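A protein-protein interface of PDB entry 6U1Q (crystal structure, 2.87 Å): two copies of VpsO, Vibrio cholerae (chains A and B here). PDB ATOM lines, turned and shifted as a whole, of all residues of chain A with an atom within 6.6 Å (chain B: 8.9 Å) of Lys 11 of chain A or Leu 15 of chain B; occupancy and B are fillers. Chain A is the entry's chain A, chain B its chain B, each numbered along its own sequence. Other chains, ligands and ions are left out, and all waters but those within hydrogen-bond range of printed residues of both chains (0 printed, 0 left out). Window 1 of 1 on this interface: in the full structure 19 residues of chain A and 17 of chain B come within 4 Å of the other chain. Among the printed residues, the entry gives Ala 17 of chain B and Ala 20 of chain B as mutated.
Of chain B, only Leu 15 comes within 4 Å of Lys 11 of chain A. No residue of chain B comes within 4 Å of Glu 10 of chain A. Of chain B, only Lys 11 and Leu 15 come within 4 Å of Glu 14 of chain A. Printed residues of chain A within 4 Å of Leu 58 of chain B: Tyr 7 (3.3 Å). Printed residues of chain B within 4 Å of Leu 15 of chain A: Leu 12, Leu 15, Thr 16 and Val 19. Printed residues of chain A within 4 Å of Thr 16 of chain B: Leu 15 (3.4 Å). Asp 9 of chain B touches none of the printed residues of chain A.
Phe 8 of chain A touches Ala 18 of chain B, and with the chains exchanged Ala 18 of chain A touches Phe 8 of chain B. Glu 14 of chain A touches Leu 15 of chain B, but with the chains exchanged Leu 15 of chain A does not touch Glu 14 of chain B (7.1 Å). Leu 15 of chain A touches Leu 12 of chain B, but with the chains exchanged Leu 12 of chain A does not touch Leu 15 of chain B (5.5 Å). Leu 15 of chain A touches its own counterpart, Leu 15 of chain B. 11 positions are printed for both chains. Of the 15 pairs that touch across the chains among the printed residues, 3 have their exchanged pair printed and touching as well.
Leu 58 of chain B touches Tyr 7 of chain A (CB to OH, 3.3 Å). Tyr 7 of chain A touches Gln 62 of chain B (CB to CG, 3.7 Å). O of Ala 18 of chain B touches CE1 of Phe 8 of chain A, at 3.96 Å. Phe 8 of chain A touches Ser 59 of chain B. Val 19 of chain B touches Leu 12 of chain A (CG1 to CD2, 3.9 Å). CD1 of Leu 15 of chain A touches CD2 of Leu 12 of chain B, 3.9 Å away. Leu 15 of chain A touches Leu 15 of chain B (N to CD1, 3.7 Å). Thr 16 of chain B touches Leu 15 of chain A (OG1 to CD1, 3.4 Å). CG1 of Val 19 of chain B touches CD2 of Leu 15 of chain A, at 3.7 Å. Ala 18 of chain A touches Phe 8 of chain B.
The side-chain amino group (NZ) of Lys 11 of chain B lies within salt-bridge range of the side-chain carboxylate (OE2) of Glu 14 of chain A.
Hydrophobic or aromatic side chains of chain A that line the printed part of chain B: Tyr 7, Phe 8, Leu 12, Leu 15 and Ala 18. Of the 24 printed residues of chain B, 11 touch a printed residue of chain A.
The side-chain hydroxyl of Ser 59 of chain B sits at hydrogen-bond distance from the backbone carbonyl oxygen of Leu 56 of chain B (3.1 Å). O of Leu 12 of chain B lies within hydrogen-bond range of OG1 of Thr 16 of chain B, at 2.7 Å. The backbone carbonyl oxygen of Ala 18 of chain B is in hydrogen-bond range of the side-chain hydroxyl of Thr 21 of chain B (2.7 Å). The side-chain hydroxyl of Thr 16 of chain A is in hydrogen-bond range of the backbone carbonyl oxygen of Leu 12 of chain A (3.2 Å). The side-chain amino group (NZ) of Lys 11 of chain A is in salt-bridge range of the side-chain carboxylate (OE1) of Glu 10 of chain A (3.3 Å).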
ATOM      1  N   ALA A   6     -37.100 -23.770 -14.938  1.00  0.00           N
ATOM      2  CA  ALA A   6     -36.987 -22.319 -15.079  1.00  0.00           C
ATOM      3  C   ALA A   6     -35.549 -21.895 -15.385  1.00  0.00           C
ATOM      4  O   ALA A   6     -35.335 -20.966 -16.177  1.00  0.00           O
ATOM      5  CB  ALA A   6     -37.515 -21.621 -13.825  1.00  0.00           C
ATOM      6  N   TYR A   7     -34.561 -22.609 -14.824  1.00  0.00           N
ATOM      7  CA  TYR A   7     -33.156 -22.225 -14.978  1.00  0.00           C
ATOM      8  C   TYR A   7     -32.668 -22.521 -16.390  1.00  0.00           C
ATOM      9  O   TYR A   7     -32.023 -21.678 -17.026  1.00  0.00           O
ATOM     10  CB  TYR A   7     -32.312 -22.999 -13.952  1.00  0.00           C
ATOM     11  CG  TYR A   7     -30.823 -22.855 -14.054  1.00  0.00           C
ATOM     12  CD1 TYR A   7     -30.178 -21.714 -13.586  1.00  0.00           C
ATOM     13  CD2 TYR A   7     -30.045 -23.878 -14.588  1.00  0.00           C
ATOM     14  CE1 TYR A   7     -28.780 -21.583 -13.673  1.00  0.00           C
ATOM     15  CE2 TYR A   7     -28.640 -23.764 -14.686  1.00  0.00           C
ATOM     16  CZ  TYR A   7     -28.020 -22.621 -14.213  1.00  0.00           C
ATOM     17  OH  TYR A   7     -26.658 -22.504 -14.309  1.00  0.00           O
ATOM     18  N   PHE A   8     -32.992 -23.708 -16.896  1.00  0.00           N
ATOM     19  CA  PHE A   8     -32.570 -24.146 -18.215  1.00  0.00           C
ATOM     20  C   PHE A   8     -33.365 -23.464 -19.317  1.00  0.00           C
ATOM     21  O   PHE A   8     -32.886 -23.352 -20.453  1.00  0.00           O
ATOM     22  CB  PHE A   8     -32.692 -25.667 -18.322  1.00  0.00           C
ATOM     23  CG  PHE A   8     -31.514 -26.408 -17.751  1.00  0.00           C
ATOM     24  CD1 PHE A   8     -30.215 -26.032 -18.097  1.00  0.00           C
ATOM     25  CD2 PHE A   8     -31.700 -27.461 -16.860  1.00  0.00           C
ATOM     26  CE1 PHE A   8     -29.115 -26.695 -17.580  1.00  0.00           C
ATOM     27  CE2 PHE A   8     -30.618 -28.122 -16.334  1.00  0.00           C
ATOM     28  CZ  PHE A   8     -29.311 -27.747 -16.710  1.00  0.00           C
ATOM     29  N   ASP A   9     -34.593 -23.043 -19.025  1.00  0.00           N
ATOM     30  CA  ASP A   9     -35.363 -22.421 -20.084  1.00  0.00           C
ATOM     31  C   ASP A   9     -34.945 -20.973 -20.323  1.00  0.00           C
ATOM     32  O   ASP A   9     -34.911 -20.551 -21.481  1.00  0.00           O
ATOM     33  CB  ASP A   9     -36.859 -22.570 -19.797  1.00  0.00           C
ATOM     34  CG  ASP A   9     -37.454 -23.829 -20.460  1.00  0.00           C
ATOM     35  OD1 ASP A   9     -37.300 -23.997 -21.698  1.00  0.00           O
ATOM     36  OD2 ASP A   9     -38.074 -24.651 -19.749  1.00  0.00           O
ATOM     37  N   GLU A  10     -34.552 -20.214 -19.286  1.00  0.00           N
ATOM     38  CA  GLU A  10     -33.928 -18.911 -19.543  1.00  0.00           C
ATOM     39  C   GLU A  10     -32.639 -19.045 -20.365  1.00  0.00           C
ATOM     40  O   GLU A  10     -32.384 -18.244 -21.278  1.00  0.00           O
ATOM     41  CB  GLU A  10     -33.668 -18.150 -18.229  1.00  0.00           C
ATOM     42  CG  GLU A  10     -32.525 -18.664 -17.309  1.00  0.00           C
ATOM     43  CD  GLU A  10     -31.109 -18.049 -17.544  1.00  0.00           C
ATOM     44  OE1 GLU A  10     -30.259 -18.207 -16.645  1.00  0.00           O
ATOM     45  OE2 GLU A  10     -30.811 -17.443 -18.600  1.00  0.00           O
ATOM     46  N   LYS A  11     -31.808 -20.052 -20.072  1.00  0.00           N
ATOM     47  CA  LYS A  11     -30.571 -20.187 -20.847  1.00  0.00           C
ATOM     48  C   LYS A  11     -30.856 -20.490 -22.298  1.00  0.00           C
ATOM     49  O   LYS A  11     -30.239 -19.883 -23.181  1.00  0.00           O
ATOM     50  CB  LYS A  11     -29.649 -21.268 -20.279  1.00  0.00           C
ATOM     51  CG  LYS A  11     -28.810 -20.799 -19.150  1.00  0.00           C
ATOM     52  CD  LYS A  11     -28.804 -21.812 -18.075  1.00  0.00           C
ATOM     53  CE  LYS A  11     -27.764 -21.456 -17.069  1.00  0.00           C
ATOM     54  NZ  LYS A  11     -27.514 -20.006 -17.073  1.00  0.00           N
ATOM     55  N   LEU A  12     -31.806 -21.414 -22.551  1.00  0.00           N
ATOM     56  CA  LEU A  12     -32.178 -21.829 -23.905  1.00  0.00           C
ATOM     57  C   LEU A  12     -32.854 -20.703 -24.657  1.00  0.00           C
ATOM     58  O   LEU A  12     -32.721 -20.593 -25.880  1.00  0.00           O
ATOM     59  CB  LEU A  12     -33.117 -23.015 -23.856  1.00  0.00           C
ATOM     60  CG  LEU A  12     -32.653 -24.455 -23.923  1.00  0.00           C
ATOM     61  CD1 LEU A  12     -33.895 -25.347 -23.695  1.00  0.00           C
ATOM     62  CD2 LEU A  12     -32.022 -24.701 -25.264  1.00  0.00           C
ATOM     63  N   ARG A  13     -33.644 -19.901 -23.956  1.00  0.00           N
ATOM     64  CA  ARG A  13     -34.268 -18.749 -24.585  1.00  0.00           C
ATOM     65  C   ARG A  13     -33.207 -17.700 -24.933  1.00  0.00           C
ATOM     66  O   ARG A  13     -33.213 -17.140 -26.039  1.00  0.00           O
ATOM     67  CB  ARG A  13     -35.364 -18.206 -23.662  1.00  0.00           C
ATOM     68  CG  ARG A  13     -35.952 -16.883 -24.067  1.00  0.00           C
ATOM     69  CD  ARG A  13     -36.962 -16.433 -23.049  1.00  0.00           C
ATOM     70  NE  ARG A  13     -36.487 -16.340 -21.655  1.00  0.00           N
ATOM     71  CZ  ARG A  13     -35.294 -15.894 -21.227  1.00  0.00           C
ATOM     72  NH1 ARG A  13     -35.054 -15.862 -19.916  1.00  0.00           N
ATOM     73  NH2 ARG A  13     -34.334 -15.487 -22.067  1.00  0.00           N
ATOM     74  N   GLU A  14     -32.265 -17.444 -23.998  1.00  0.00           N
ATOM     75  CA  GLU A  14     -31.199 -16.480 -24.242  1.00  0.00           C
ATOM     76  C   GLU A  14     -30.284 -16.949 -25.368  1.00  0.00           C
ATOM     77  O   GLU A  14     -29.936 -16.156 -26.260  1.00  0.00           O
ATOM     78  CB  GLU A  14     -30.392 -16.269 -22.971  1.00  0.00           C
ATOM     79  CG  GLU A  14     -29.715 -14.892 -22.866  1.00  0.00           C
ATOM     80  CD  GLU A  14     -28.965 -14.679 -21.518  1.00  0.00           C
ATOM     81  OE1 GLU A  14     -29.116 -15.512 -20.587  1.00  0.00           O
ATOM     82  OE2 GLU A  14     -28.223 -13.675 -21.388  1.00  0.00           O
ATOM     83  N   LEU A  15     -29.945 -18.255 -25.393  1.00  0.00           N
ATOM     84  CA  LEU A  15     -29.095 -18.773 -26.462  1.00  0.00           C
ATOM     85  C   LEU A  15     -29.783 -18.656 -27.816  1.00  0.00           C
ATOM     86  O   LEU A  15     -29.183 -18.167 -28.778  1.00  0.00           O
ATOM     87  CB  LEU A  15     -28.684 -20.220 -26.185  1.00  0.00           C
ATOM     88  CG  LEU A  15     -27.883 -21.072 -27.235  1.00  0.00           C
ATOM     89  CD1 LEU A  15     -26.590 -20.473 -27.820  1.00  0.00           C
ATOM     90  CD2 LEU A  15     -27.526 -22.415 -26.668  1.00  0.00           C
ATOM     91  N   THR A  16     -31.058 -19.054 -27.905  1.00  0.00           N
ATOM     92  CA  THR A  16     -31.796 -18.915 -29.166  1.00  0.00           C
ATOM     93  C   THR A  16     -31.870 -17.444 -29.592  1.00  0.00           C
ATOM     94  O   THR A  16     -31.588 -17.106 -30.751  1.00  0.00           O
ATOM     95  CB  THR A  16     -33.215 -19.533 -29.045  1.00  0.00           C
ATOM     96  OG1 THR A  16     -33.167 -20.973 -28.976  1.00  0.00           O
ATOM     97  CG2 THR A  16     -34.118 -19.144 -30.235  1.00  0.00           C
ATOM     98  N   ALA A  18     -29.830 -14.967 -28.790  1.00  0.00           N
ATOM     99  CA  ALA A  18     -28.528 -14.484 -29.230  1.00  0.00           C
ATOM    100  C   ALA A  18     -28.206 -14.980 -30.640  1.00  0.00           C
ATOM    101  O   ALA A  18     -27.787 -14.202 -31.508  1.00  0.00           O
ATOM    102  CB  ALA A  18     -27.443 -14.911 -28.241  1.00  0.00           C
ATOM    103  N   TYR B   7     -17.262  -9.675 -25.435  1.00  0.00           N
ATOM    104  CA  TYR B   7     -18.215 -10.317 -24.519  1.00  0.00           C
ATOM    105  C   TYR B   7     -19.263 -11.213 -25.192  1.00  0.00           C
ATOM    106  O   TYR B   7     -19.642 -12.245 -24.623  1.00  0.00           O
ATOM    107  CB  TYR B   7     -18.902  -9.222 -23.683  1.00  0.00           C
ATOM    108  CG  TYR B   7     -20.113  -9.663 -22.896  1.00  0.00           C
ATOM    109  CD1 TYR B   7     -19.986 -10.143 -21.594  1.00  0.00           C
ATOM    110  CD2 TYR B   7     -21.396  -9.574 -23.444  1.00  0.00           C
ATOM    111  CE1 TYR B   7     -21.103 -10.549 -20.856  1.00  0.00           C
ATOM    112  CE2 TYR B   7     -22.521  -9.990 -22.724  1.00  0.00           C
ATOM    113  CZ  TYR B   7     -22.366 -10.470 -21.429  1.00  0.00           C
ATOM    114  OH  TYR B   7     -23.478 -10.869 -20.726  1.00  0.00           O
ATOM    115  N   PHE B   8     -19.785 -10.837 -26.368  1.00  0.00           N
ATOM    116  CA  PHE B   8     -20.927 -11.566 -26.930  1.00  0.00           C
ATOM    117  C   PHE B   8     -20.583 -13.018 -27.290  1.00  0.00           C
ATOM    118  O   PHE B   8     -21.440 -13.906 -27.181  1.00  0.00           O
ATOM    119  CB  PHE B   8     -21.436 -10.818 -28.170  1.00  0.00           C
ATOM    120  CG  PHE B   8     -22.593 -11.502 -28.883  1.00  0.00           C
ATOM    121  CD1 PHE B   8     -22.403 -12.134 -30.116  1.00  0.00           C
ATOM    122  CD2 PHE B   8     -23.879 -11.492 -28.330  1.00  0.00           C
ATOM    123  CE1 PHE B   8     -23.477 -12.750 -30.799  1.00  0.00           C
ATOM    124  CE2 PHE B   8     -24.948 -12.121 -28.988  1.00  0.00           C
ATOM    125  CZ  PHE B   8     -24.747 -12.749 -30.233  1.00  0.00           C
ATOM    126  N   ASP B   9     -19.324 -13.290 -27.665  1.00  0.00           N
ATOM    127  CA  ASP B   9     -18.905 -14.639 -28.043  1.00  0.00           C
ATOM    128  C   ASP B   9     -18.655 -15.526 -26.825  1.00  0.00           C
ATOM    129  O   ASP B   9     -18.923 -16.737 -26.889  1.00  0.00           O
ATOM    130  CB  ASP B   9     -17.665 -14.555 -28.927  1.00  0.00           C
ATOM    131  CG  ASP B   9     -17.947 -13.873 -30.258  1.00  0.00           C
ATOM    132  OD1 ASP B   9     -18.870 -14.315 -30.998  1.00  0.00           O
ATOM    133  OD2 ASP B   9     -17.241 -12.884 -30.555  1.00  0.00           O
ATOM    134  N   GLU B  10     -18.154 -14.934 -25.723  1.00  0.00           N
ATOM    135  CA  GLU B  10     -18.152 -15.593 -24.415  1.00  0.00           C
ATOM    136  C   GLU B  10     -19.566 -15.984 -24.006  1.00  0.00           C
ATOM    137  O   GLU B  10     -19.780 -17.054 -23.428  1.00  0.00           O
ATOM    138  CB  GLU B  10     -17.565 -14.671 -23.339  1.00  0.00           C
ATOM    139  CG  GLU B  10     -16.330 -13.863 -23.737  1.00  0.00           C
ATOM    140  CD  GLU B  10     -15.483 -13.424 -22.529  1.00  0.00           C
ATOM    141  OE1 GLU B  10     -15.939 -13.594 -21.375  1.00  0.00           O
ATOM    142  OE2 GLU B  10     -14.360 -12.908 -22.739  1.00  0.00           O
ATOM    143  N   LYS B  11     -20.545 -15.113 -24.291  1.00  0.00           N
ATOM    144  CA  LYS B  11     -21.949 -15.405 -23.997  1.00  0.00           C
ATOM    145  C   LYS B  11     -22.457 -16.606 -24.807  1.00  0.00           C
ATOM    146  O   LYS B  11     -23.184 -17.458 -24.275  1.00  0.00           O
ATOM    147  CB  LYS B  11     -22.782 -14.143 -24.259  1.00  0.00           C
ATOM    148  CG  LYS B  11     -24.191 -14.121 -23.694  1.00  0.00           C
ATOM    149  CD  LYS B  11     -24.991 -12.982 -24.332  1.00  0.00           C
ATOM    150  CE  LYS B  11     -26.507 -13.191 -24.194  1.00  0.00           C
ATOM    151  NZ  LYS B  11     -27.293 -11.909 -24.252  1.00  0.00           N
ATOM    152  N   LEU B  12     -22.088 -16.686 -26.100  1.00  0.00           N
ATOM    153  CA  LEU B  12     -22.468 -17.833 -26.929  1.00  0.00           C
ATOM    154  C   LEU B  12     -21.765 -19.119 -26.501  1.00  0.00           C
ATOM    155  O   LEU B  12     -22.386 -20.194 -26.470  1.00  0.00           O
ATOM    156  CB  LEU B  12     -22.141 -17.553 -28.391  1.00  0.00           C
ATOM    157  CG  LEU B  12     -23.202 -16.728 -29.121  1.00  0.00           C
ATOM    158  CD1 LEU B  12     -22.664 -16.151 -30.409  1.00  0.00           C
ATOM    159  CD2 LEU B  12     -24.457 -17.549 -29.396  1.00  0.00           C
ATOM    160  N   ARG B  13     -20.480 -19.033 -26.142  1.00  0.00           N
ATOM    161  CA  ARG B  13     -19.769 -20.246 -25.770  1.00  0.00           C
ATOM    162  C   ARG B  13     -20.304 -20.800 -24.469  1.00  0.00           C
ATOM    163  O   ARG B  13     -20.686 -21.973 -24.392  1.00  0.00           O
ATOM    164  CB  ARG B  13     -18.269 -19.977 -25.652  1.00  0.00           C
ATOM    165  CG  ARG B  13     -17.464 -20.140 -26.941  1.00  0.00           C
ATOM    166  CD  ARG B  13     -15.956 -20.126 -26.655  1.00  0.00           C
ATOM    167  NE  ARG B  13     -15.543 -19.052 -25.747  1.00  0.00           N
ATOM    168  CZ  ARG B  13     -15.336 -17.787 -26.116  1.00  0.00           C
ATOM    169  NH1 ARG B  13     -15.530 -17.414 -27.380  1.00  0.00           N
ATOM    170  NH2 ARG B  13     -14.955 -16.889 -25.214  1.00  0.00           N
ATOM    171  N   GLU B  14     -20.376 -19.968 -23.443  1.00  0.00           N
ATOM    172  CA  GLU B  14     -20.804 -20.487 -22.151  1.00  0.00           C
ATOM    173  C   GLU B  14     -22.290 -20.791 -22.105  1.00  0.00           C
ATOM    174  O   GLU B  14     -22.677 -21.679 -21.343  1.00  0.00           O
ATOM    175  CB  GLU B  14     -20.364 -19.589 -20.973  1.00  0.00           C
ATOM    176  CG  GLU B  14     -20.815 -18.160 -20.902  1.00  0.00           C
ATOM    177  CD  GLU B  14     -21.048 -17.717 -19.480  1.00  0.00           C
ATOM    178  OE1 GLU B  14     -21.536 -16.585 -19.295  1.00  0.00           O
ATOM    179  OE2 GLU B  14     -20.768 -18.503 -18.551  1.00  0.00           O
ATOM    180  N   LEU B  15     -23.131 -20.038 -22.833  1.00  0.00           N
ATOM    181  CA  LEU B  15     -24.545 -20.406 -22.924  1.00  0.00           C
ATOM    182  C   LEU B  15     -24.703 -21.769 -23.595  1.00  0.00           C
ATOM    183  O   LEU B  15     -25.491 -22.603 -23.137  1.00  0.00           O
ATOM    184  CB  LEU B  15     -25.340 -19.339 -23.683  1.00  0.00           C
ATOM    185  CG  LEU B  15     -26.079 -18.196 -22.956  1.00  0.00           C
ATOM    186  CD1 LEU B  15     -26.729 -17.228 -23.972  1.00  0.00           C
ATOM    187  CD2 LEU B  15     -27.089 -18.666 -21.866  1.00  0.00           C
ATOM    188  N   THR B  16     -23.957 -22.004 -24.686  1.00  0.00           N
ATOM    189  CA  THR B  16     -23.975 -23.290 -25.379  1.00  0.00           C
ATOM    190  C   THR B  16     -23.500 -24.413 -24.476  1.00  0.00           C
ATOM    191  O   THR B  16     -24.100 -25.498 -24.420  1.00  0.00           O
ATOM    192  CB  THR B  16     -23.089 -23.209 -26.606  1.00  0.00           C
ATOM    193  OG1 THR B  16     -23.709 -22.328 -27.534  1.00  0.00           O
ATOM    194  CG2 THR B  16     -22.839 -24.608 -27.231  1.00  0.00           C
ATOM    195  N   ALA B  17     -22.400 -24.171 -23.780  1.00  0.00           N
ATOM    196  CA  ALA B  17     -21.876 -25.158 -22.857  1.00  0.00           C
ATOM    197  C   ALA B  17     -22.952 -25.598 -21.876  1.00  0.00           C
ATOM    198  O   ALA B  17     -23.059 -26.780 -21.560  1.00  0.00           O
ATOM    199  CB  ALA B  17     -20.660 -24.566 -22.135  1.00  0.00           C
ATOM    200  N   ALA B  18     -23.756 -24.648 -21.385  1.00  0.00           N
ATOM    201  CA  ALA B  18     -24.813 -24.949 -20.414  1.00  0.00           C
ATOM    202  C   ALA B  18     -25.869 -25.896 -20.982  1.00  0.00           C
ATOM    203  O   ALA B  18     -26.258 -26.865 -20.319  1.00  0.00           O
ATOM    204  CB  ALA B  18     -25.474 -23.654 -19.926  1.00  0.00           C
ATOM    205  N   VAL B  19     -26.377 -25.615 -22.188  1.00  0.00           N
ATOM    206  CA  VAL B  19     -27.413 -26.490 -22.737  1.00  0.00           C
ATOM    207  C   VAL B  19     -26.825 -27.857 -23.088  1.00  0.00           C
ATOM    208  O   VAL B  19     -27.532 -28.873 -23.054  1.00  0.00           O
ATOM    209  CB  VAL B  19     -28.143 -25.842 -23.942  1.00  0.00           C
ATOM    210  CG1 VAL B  19     -28.453 -24.352 -23.653  1.00  0.00           C
ATOM    211  CG2 VAL B  19     -27.371 -26.063 -25.273  1.00  0.00           C
ATOM    212  N   ALA B  20     -25.536 -27.920 -23.408  1.00  0.00           N
ATOM    213  CA  ALA B  20     -24.934 -29.211 -23.708  1.00  0.00           C
ATOM    214  C   ALA B  20     -24.931 -30.145 -22.508  1.00  0.00           C
ATOM    215  O   ALA B  20     -24.617 -31.332 -22.677  1.00  0.00           O
ATOM    216  CB  ALA B  20     -23.490 -29.042 -24.212  1.00  0.00           C
ATOM    217  N   THR B  21     -25.212 -29.635 -21.306  1.00  0.00           N
ATOM    218  CA  THR B  21     -25.227 -30.444 -20.094  1.00  0.00           C
ATOM    219  C   THR B  21     -26.629 -30.674 -19.532  1.00  0.00           C
ATOM    220  O   THR B  21     -26.748 -31.192 -18.420  1.00  0.00           O
ATOM    221  CB  THR B  21     -24.350 -29.812 -19.016  1.00  0.00           C
ATOM    222  OG1 THR B  21     -24.831 -28.502 -18.717  1.00  0.00           O
ATOM    223  CG2 THR B  21     -22.918 -29.728 -19.479  1.00  0.00           C
ATOM    224  N   ILE B  22     -27.690 -30.309 -20.259  1.00  0.00           N
ATOM    225  CA  ILE B  22     -29.028 -30.408 -19.691  1.00  0.00           C
ATOM    226  C   ILE B  22     -29.457 -31.857 -19.537  1.00  0.00           C
ATOM    227  O   ILE B  22     -29.903 -32.258 -18.465  1.00  0.00           O
ATOM    228  CB  ILE B  22     -30.061 -29.657 -20.538  1.00  0.00           C
ATOM    229  CG1 ILE B  22     -29.668 -28.206 -20.764  1.00  0.00           C
ATOM    230  CG2 ILE B  22     -31.377 -29.749 -19.831  1.00  0.00           C
ATOM    231  CD1 ILE B  22     -30.793 -27.341 -21.264  1.00  0.00           C
ATOM    232  N   THR B  51     -15.811 -26.580 -17.712  1.00  0.00           N
ATOM    233  CA  THR B  51     -17.061 -25.811 -17.810  1.00  0.00           C
ATOM    234  C   THR B  51     -18.296 -26.708 -17.768  1.00  0.00           C
ATOM    235  O   THR B  51     -19.357 -26.275 -17.294  1.00  0.00           O
ATOM    236  CB  THR B  51     -17.108 -24.912 -19.050  1.00  0.00           C
ATOM    237  OG1 THR B  51     -17.024 -25.698 -20.235  1.00  0.00           O
ATOM    238  CG2 THR B  51     -15.997 -23.868 -19.004  1.00  0.00           C
ATOM    239  N   LEU B  54     -18.957 -27.174 -13.769  1.00  0.00           N
ATOM    240  CA  LEU B  54     -19.658 -26.092 -13.083  1.00  0.00           C
ATOM    241  C   LEU B  54     -21.080 -25.980 -13.594  1.00  0.00           C
ATOM    242  O   LEU B  54     -22.013 -25.803 -12.808  1.00  0.00           O
ATOM    243  CB  LEU B  54     -18.911 -24.757 -13.208  1.00  0.00           C
ATOM    244  CG  LEU B  54     -18.729 -24.043 -14.545  1.00  0.00           C
ATOM    245  CD1 LEU B  54     -19.678 -22.837 -14.732  1.00  0.00           C
ATOM    246  CD2 LEU B  54     -17.272 -23.628 -14.664  1.00  0.00           C
ATOM    247  N   ASN B  55     -21.258 -26.049 -14.913  1.00  0.00           N
ATOM    248  CA  ASN B  55     -22.601 -25.942 -15.471  1.00  0.00           C
ATOM    249  C   ASN B  55     -23.527 -27.030 -14.938  1.00  0.00           C
ATOM    250  O   ASN B  55     -24.701 -26.767 -14.648  1.00  0.00           O
ATOM    251  CB  ASN B  55     -22.532 -25.983 -16.987  1.00  0.00           C
ATOM    252  CG  ASN B  55     -22.645 -24.618 -17.576  1.00  0.00           C
ATOM    253  OD1 ASN B  55     -23.523 -23.840 -17.182  1.00  0.00           O
ATOM    254  ND2 ASN B  55     -21.751 -24.291 -18.498  1.00  0.00           N
ATOM    255  N   LEU B  56     -23.017 -28.250 -14.794  1.00  0.00           N
ATOM    256  CA  LEU B  56     -23.811 -29.304 -14.183  1.00  0.00           C
ATOM    257  C   LEU B  56     -24.141 -28.961 -12.742  1.00  0.00           C
ATOM    258  O   LEU B  56     -25.302 -29.005 -12.322  1.00  0.00           O
ATOM    259  CB  LEU B  56     -23.062 -30.626 -14.250  1.00  0.00           C
ATOM    260  CG  LEU B  56     -23.897 -31.784 -13.759  1.00  0.00           C
ATOM    261  CD1 LEU B  56     -25.061 -31.869 -14.709  1.00  0.00           C
ATOM    262  CD2 LEU B  56     -23.080 -33.043 -13.801  1.00  0.00           C
ATOM    263  N   LEU B  58     -24.095 -26.110 -11.266  1.00  0.00           N
ATOM    264  CA  LEU B  58     -24.940 -24.929 -11.154  1.00  0.00           C
ATOM    265  C   LEU B  58     -26.405 -25.299 -11.311  1.00  0.00           C
ATOM    266  O   LEU B  58     -27.269 -24.797 -10.579  1.00  0.00           O
ATOM    267  CB  LEU B  58     -24.531 -23.891 -12.200  1.00  0.00           C
ATOM    268  CG  LEU B  58     -23.282 -23.057 -11.884  1.00  0.00           C
ATOM    269  CD1 LEU B  58     -22.768 -22.332 -13.123  1.00  0.00           C
ATOM    270  CD2 LEU B  58     -23.551 -22.076 -10.744  1.00  0.00           C
ATOM    271  N   SER B  59     -26.709 -26.200 -12.236  1.00  0.00           N
ATOM    272  CA  SER B  59     -28.114 -26.529 -12.402  1.00  0.00           C
ATOM    273  C   SER B  59     -28.608 -27.462 -11.302  1.00  0.00           C
ATOM    274  O   SER B  59     -29.709 -27.270 -10.784  1.00  0.00           O
ATOM    275  CB  SER B  59     -28.351 -27.138 -13.769  1.00  0.00           C
ATOM    276  OG  SER B  59     -27.933 -28.480 -13.803  1.00  0.00           O
ATOM    277  N   GLN B  62     -30.175 -25.907  -8.307  1.00  0.00           N
ATOM    278  CA  GLN B  62     -31.535 -25.393  -8.287  1.00  0.00           C
ATOM    279  C   GLN B  62     -32.451 -26.228  -7.407  1.00  0.00           C
ATOM    280  O   GLN B  62     -33.373 -25.681  -6.792  1.00  0.00           O
ATOM    281  CB  GLN B  62     -32.132 -25.390  -9.696  1.00  0.00           C
ATOM    282  CG  GLN B  62     -31.500 -24.438 -10.660  1.00  0.00           C
ATOM    283  CD  GLN B  62     -31.350 -23.048 -10.092  1.00  0.00           C
ATOM    284  OE1 GLN B  62     -32.279 -22.217 -10.181  1.00  0.00           O
ATOM    285  NE2 GLN B  62     -30.167 -22.772  -9.494  1.00  0.00           N
ATOM    286  N   GLN B 110     -25.328 -16.227  -5.505  1.00  0.00           N
ATOM    287  CA  GLN B 110     -26.096 -15.979  -6.718  1.00  0.00           C
ATOM    288  C   GLN B 110     -26.881 -17.226  -7.107  1.00  0.00           C
ATOM    289  O   GLN B 110     -27.975 -17.124  -7.680  1.00  0.00           O
ATOM    290  CB  GLN B 110     -25.154 -15.541  -7.854  1.00  0.00           C
ATOM    291  CG  GLN B 110     -25.670 -15.715  -9.307  1.00  0.00           C
ATOM    292  CD  GLN B 110     -25.571 -17.159  -9.827  1.00  0.00           C
ATOM    293  OE1 GLN B 110     -26.587 -17.809 -10.094  1.00  0.00           O
ATOM    294  NE2 GLN B 110     -24.343 -17.670  -9.942  1.00  0.00           N
